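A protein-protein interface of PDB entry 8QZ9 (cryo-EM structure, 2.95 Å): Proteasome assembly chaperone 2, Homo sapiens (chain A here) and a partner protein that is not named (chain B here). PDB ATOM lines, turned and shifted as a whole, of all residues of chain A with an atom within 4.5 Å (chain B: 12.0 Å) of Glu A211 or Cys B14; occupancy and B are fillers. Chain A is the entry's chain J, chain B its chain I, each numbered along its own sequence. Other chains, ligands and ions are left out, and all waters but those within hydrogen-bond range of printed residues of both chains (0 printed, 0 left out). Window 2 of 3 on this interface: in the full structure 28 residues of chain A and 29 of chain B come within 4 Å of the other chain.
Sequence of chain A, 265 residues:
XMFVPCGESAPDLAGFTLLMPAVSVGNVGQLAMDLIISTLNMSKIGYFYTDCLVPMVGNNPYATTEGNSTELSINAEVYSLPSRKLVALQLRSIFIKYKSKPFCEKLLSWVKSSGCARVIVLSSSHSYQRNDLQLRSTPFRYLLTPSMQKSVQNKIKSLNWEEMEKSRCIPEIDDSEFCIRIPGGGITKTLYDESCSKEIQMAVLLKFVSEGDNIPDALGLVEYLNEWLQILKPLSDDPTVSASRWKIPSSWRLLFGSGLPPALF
The side-chain carboxylate (OE2) of Glu A211 lies within hydrogen-bond range of the side-chain sulfur (SG) of Cys B14 (3.2 Å).
The guanidinium group of Arg B15 is in salt-bridge range of the side-chain carboxylate of Glu A211 (3.5 Å).
NH2 of Arg B15 sits at hydrogen-bond distance from OD1 of Asn A214 (3.4 Å).
Among the printed residues, pairs that only touch across the chains: Gly A26 with Arg B15 and Gly A212 with Arg B15.
Among the printed residues, 5 pairs touch across the chains.
Among the printed residues, Asp or Glu carboxylates within 4 Å of a Lys or Arg side-chain nitrogen of the other chain: Glu A211 with Arg B15 (3.5 Å).
Gly A26 touches just one residue of chain B: Arg B15.
No residue of chain B comes within 4 Å of Ser A210.
Of the printed residues of chain B, Glu A211 touches Cys B14 (3.2 Å) and Arg B15 (3.4 Å).
Of chain B, only Arg B15 comes within 4 Å of Gly A212.
Of the printed residues of chain B, Asn A214 touches Arg B15.
Cys B14 touches just one residue of chain A: Glu A211.
Of the printed residues of chain A, Arg B15 touches Gly A26, Glu A211, Gly A212 and Asn A214.
The nearest residue of chain A that does not touch Cys B14 is Val A25 (4.3 Å).
The backbone carbonyl oxygen (O) of Ser A210 sits at hydrogen-bond distance from the side-chain amide nitrogen (ND2) of Asn A214.
O of Gly A212 lies close to OD1 of Asn A214 (2.9 Å).
The side-chain sulfur (SG) of Cys B14 lies close to the backbone NH (N) of Ala B16 (3.8 Å).
SG of Cys B14 is in hydrogen-bond range of OG1 of Thr B18.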
ATOM      1  N   VAL A  25     -23.066  19.829   7.854  1.00  0.00           N
ATOM      2  CA  VAL A  25     -21.621  19.830   8.042  1.00  0.00           C
ATOM      3  C   VAL A  25     -21.208  18.628   8.881  1.00  0.00           C
ATOM      4  O   VAL A  25     -21.767  18.372   9.954  1.00  0.00           O
ATOM      5  CB  VAL A  25     -21.162  21.154   8.673  1.00  0.00           C
ATOM      6  CG1 VAL A  25     -21.896  21.423   9.973  1.00  0.00           C
ATOM      7  CG2 VAL A  25     -19.665  21.133   8.916  1.00  0.00           C
ATOM      8  N   GLY A  26     -20.241  17.866   8.377  1.00  0.00           N
ATOM      9  CA  GLY A  26     -19.685  16.746   9.104  1.00  0.00           C
ATOM     10  C   GLY A  26     -20.476  15.457   9.037  1.00  0.00           C
ATOM     11  O   GLY A  26     -20.023  14.452   9.597  1.00  0.00           O
ATOM     12  N   SER A 210     -17.281  20.694  13.840  1.00  0.00           N
ATOM     13  CA  SER A 210     -16.270  21.076  12.866  1.00  0.00           C
ATOM     14  C   SER A 210     -15.822  19.834  12.108  1.00  0.00           C
ATOM     15  O   SER A 210     -15.974  18.706  12.582  1.00  0.00           O
ATOM     16  CB  SER A 210     -15.070  21.758  13.531  1.00  0.00           C
ATOM     17  OG  SER A 210     -15.458  22.967  14.157  1.00  0.00           O
ATOM     18  N   GLU A 211     -15.265  20.052  10.920  1.00  0.00           N
ATOM     19  CA  GLU A 211     -14.897  18.945  10.049  1.00  0.00           C
ATOM     20  C   GLU A 211     -13.706  18.171  10.604  1.00  0.00           C
ATOM     21  O   GLU A 211     -12.812  18.731  11.243  1.00  0.00           O
ATOM     22  CB  GLU A 211     -14.575  19.454   8.647  1.00  0.00           C
ATOM     23  CG  GLU A 211     -15.711  20.214   7.993  1.00  0.00           C
ATOM     24  CD  GLU A 211     -16.573  19.328   7.122  1.00  0.00           C
ATOM     25  OE1 GLU A 211     -16.548  18.097   7.319  1.00  0.00           O
ATOM     26  OE2 GLU A 211     -17.275  19.862   6.238  1.00  0.00           O
ATOM     27  N   GLY A 212     -13.702  16.867  10.341  1.00  0.00           N
ATOM     28  CA  GLY A 212     -12.669  15.979  10.837  1.00  0.00           C
ATOM     29  C   GLY A 212     -13.247  14.665  11.320  1.00  0.00           C
ATOM     30  O   GLY A 212     -14.245  14.188  10.773  1.00  0.00           O
ATOM     31  N   ASN A 214     -15.605  12.816  13.196  1.00  0.00           N
ATOM     32  CA  ASN A 214     -16.895  13.236  13.731  1.00  0.00           C
ATOM     33  C   ASN A 214     -17.698  12.063  14.284  1.00  0.00           C
ATOM     34  O   ASN A 214     -18.925  12.044  14.185  1.00  0.00           O
ATOM     35  CB  ASN A 214     -17.700  13.976  12.666  1.00  0.00           C
ATOM     36  CG  ASN A 214     -17.166  15.366  12.394  1.00  0.00           C
ATOM     37  OD1 ASN A 214     -16.692  15.658  11.298  1.00  0.00           O
ATOM     38  ND2 ASN A 214     -17.246  16.235  13.393  1.00  0.00           N
ATOM     39  N   ALA B   2      -5.536  29.234  -0.212  1.00  0.00           N
ATOM     40  CA  ALA B   2      -6.512  30.128  -0.820  1.00  0.00           C
ATOM     41  C   ALA B   2      -6.326  31.556  -0.319  1.00  0.00           C
ATOM     42  O   ALA B   2      -7.244  32.372  -0.391  1.00  0.00           O
ATOM     43  CB  ALA B   2      -7.924  29.646  -0.538  1.00  0.00           C
ATOM     44  N   VAL B  10      -9.440  33.056   5.631  1.00  0.00           N
ATOM     45  CA  VAL B  10      -9.957  32.032   4.734  1.00  0.00           C
ATOM     46  C   VAL B  10     -10.763  31.025   5.540  1.00  0.00           C
ATOM     47  O   VAL B  10     -10.503  30.792   6.724  1.00  0.00           O
ATOM     48  CB  VAL B  10      -8.826  31.327   3.957  1.00  0.00           C
ATOM     49  CG1 VAL B  10      -8.154  32.301   3.009  1.00  0.00           C
ATOM     50  CG2 VAL B  10      -7.816  30.730   4.920  1.00  0.00           C
ATOM     51  N   LYS B  11     -11.752  30.425   4.883  1.00  0.00           N
ATOM     52  CA  LYS B  11     -12.632  29.442   5.496  1.00  0.00           C
ATOM     53  C   LYS B  11     -12.368  28.068   4.898  1.00  0.00           C
ATOM     54  O   LYS B  11     -12.155  27.937   3.690  1.00  0.00           O
ATOM     55  CB  LYS B  11     -14.101  29.826   5.302  1.00  0.00           C
ATOM     56  N   ALA B  12     -12.381  27.048   5.753  1.00  0.00           N
ATOM     57  CA  ALA B  12     -12.102  25.694   5.310  1.00  0.00           C
ATOM     58  C   ALA B  12     -13.232  25.173   4.423  1.00  0.00           C
ATOM     59  O   ALA B  12     -14.392  25.557   4.590  1.00  0.00           O
ATOM     60  CB  ALA B  12     -11.915  24.772   6.511  1.00  0.00           C
ATOM     61  N   PRO B  13     -12.921  24.295   3.472  1.00  0.00           N
ATOM     62  CA  PRO B  13     -13.963  23.753   2.597  1.00  0.00           C
ATOM     63  C   PRO B  13     -14.853  22.759   3.327  1.00  0.00           C
ATOM     64  O   PRO B  13     -14.488  22.188   4.356  1.00  0.00           O
ATOM     65  CB  PRO B  13     -13.167  23.070   1.482  1.00  0.00           C
ATOM     66  CG  PRO B  13     -11.894  22.676   2.141  1.00  0.00           C
ATOM     67  CD  PRO B  13     -11.588  23.765   3.132  1.00  0.00           C
ATOM     68  N   CYS B  14     -16.043  22.555   2.769  1.00  0.00           N
ATOM     69  CA  CYS B  14     -17.034  21.642   3.322  1.00  0.00           C
ATOM     70  C   CYS B  14     -17.224  20.466   2.376  1.00  0.00           C
ATOM     71  O   CYS B  14     -17.450  20.660   1.177  1.00  0.00           O
ATOM     72  CB  CYS B  14     -18.367  22.357   3.555  1.00  0.00           C
ATOM     73  SG  CYS B  14     -19.537  21.447   4.586  1.00  0.00           S
ATOM     74  N   ARG B  15     -17.136  19.251   2.914  1.00  0.00           N
ATOM     75  CA  ARG B  15     -17.262  18.046   2.108  1.00  0.00           C
ATOM     76  C   ARG B  15     -18.704  17.665   1.815  1.00  0.00           C
ATOM     77  O   ARG B  15     -18.936  16.782   0.983  1.00  0.00           O
ATOM     78  CB  ARG B  15     -16.561  16.869   2.796  1.00  0.00           C
ATOM     79  CG  ARG B  15     -17.225  16.407   4.077  1.00  0.00           C
ATOM     80  CD  ARG B  15     -16.584  15.132   4.595  1.00  0.00           C
ATOM     81  NE  ARG B  15     -17.049  14.789   5.933  1.00  0.00           N
ATOM     82  CZ  ARG B  15     -16.274  14.747   7.007  1.00  0.00           C
ATOM     83  NH1 ARG B  15     -14.983  15.025   6.938  1.00  0.00           N
ATOM     84  NH2 ARG B  15     -16.807  14.421   8.180  1.00  0.00           N
ATOM     85  N   ALA B  16     -19.674  18.296   2.472  1.00  0.00           N
ATOM     86  CA  ALA B  16     -21.082  17.999   2.253  1.00  0.00           C
ATOM     87  C   ALA B  16     -21.720  18.888   1.196  1.00  0.00           C
ATOM     88  O   ALA B  16     -22.903  18.713   0.893  1.00  0.00           O
ATOM     89  CB  ALA B  16     -21.858  18.124   3.566  1.00  0.00           C
ATOM     90  N   GLY B  17     -20.971  19.831   0.631  1.00  0.00           N
ATOM     91  CA  GLY B  17     -21.490  20.697  -0.410  1.00  0.00           C
ATOM     92  C   GLY B  17     -22.608  21.612   0.042  1.00  0.00           C
ATOM     93  O   GLY B  17     -23.606  21.779  -0.664  1.00  0.00           O
ATOM     94  N   THR B  18     -22.454  22.215   1.221  1.00  0.00           N
ATOM     95  CA  THR B  18     -23.428  23.162   1.752  1.00  0.00           C
ATOM     96  C   THR B  18     -22.965  24.606   1.600  1.00  0.00           C
ATOM     97  O   THR B  18     -23.552  25.509   2.203  1.00  0.00           O
ATOM     98  CB  THR B  18     -23.725  22.856   3.221  1.00  0.00           C
ATOM     99  OG1 THR B  18     -22.528  23.003   3.995  1.00  0.00           O
ATOM    100  CG2 THR B  18     -24.247  21.439   3.374  1.00  0.00           C
ATOM    101  N   GLU B  19     -21.926  24.842   0.800  1.00  0.00           N
ATOM    102  CA  GLU B  19     -21.349  26.168   0.639  1.00  0.00           C
ATOM    103  C   GLU B  19     -22.135  27.059  -0.313  1.00  0.00           C
ATOM    104  O   GLU B  19     -21.836  28.254  -0.400  1.00  0.00           O
ATOM    105  CB  GLU B  19     -19.899  26.048   0.154  1.00  0.00           C
ATOM    106  CG  GLU B  19     -19.736  25.337  -1.185  1.00  0.00           C
ATOM    107  CD  GLU B  19     -19.849  26.273  -2.374  1.00  0.00           C
ATOM    108  OE1 GLU B  19     -19.672  27.495  -2.189  1.00  0.00           O
ATOM    109  OE2 GLU B  19     -20.114  25.785  -3.492  1.00  0.00           O
ATOM    110  N   ASP B  20     -23.125  26.518  -1.024  1.00  0.00           N
ATOM    111  CA  ASP B  20     -23.895  27.328  -1.961  1.00  0.00           C
ATOM    112  C   ASP B  20     -24.889  28.251  -1.268  1.00  0.00           C
ATOM    113  O   ASP B  20     -25.508  29.080  -1.945  1.00  0.00           O
ATOM    114  CB  ASP B  20     -24.623  26.426  -2.964  1.00  0.00           C
ATOM    115  CG  ASP B  20     -25.641  25.506  -2.307  1.00  0.00           C
ATOM    116  OD1 ASP B  20     -25.770  25.523  -1.064  1.00  0.00           O
ATOM    117  OD2 ASP B  20     -26.320  24.761  -3.043  1.00  0.00           O
ATOM    118  N   GLU B  21     -25.063  28.117   0.043  1.00  0.00           N
ATOM    119  CA  GLU B  21     -25.985  28.940   0.836  1.00  0.00           C
ATOM    120  C   GLU B  21     -27.406  28.697   0.320  1.00  0.00           C
ATOM    121  O   GLU B  21     -27.719  27.610  -0.182  1.00  0.00           O
ATOM    122  CB  GLU B  21     -25.537  30.392   0.810  1.00  0.00           C
ATOM    123  CG  GLU B  21     -24.133  30.617   1.344  1.00  0.00           C
ATOM    124  CD  GLU B  21     -24.009  31.905   2.130  1.00  0.00           C
ATOM    125  OE1 GLU B  21     -23.149  31.970   3.035  1.00  0.00           O
ATOM    126  OE2 GLU B  21     -24.767  32.853   1.843  1.00  0.00           O
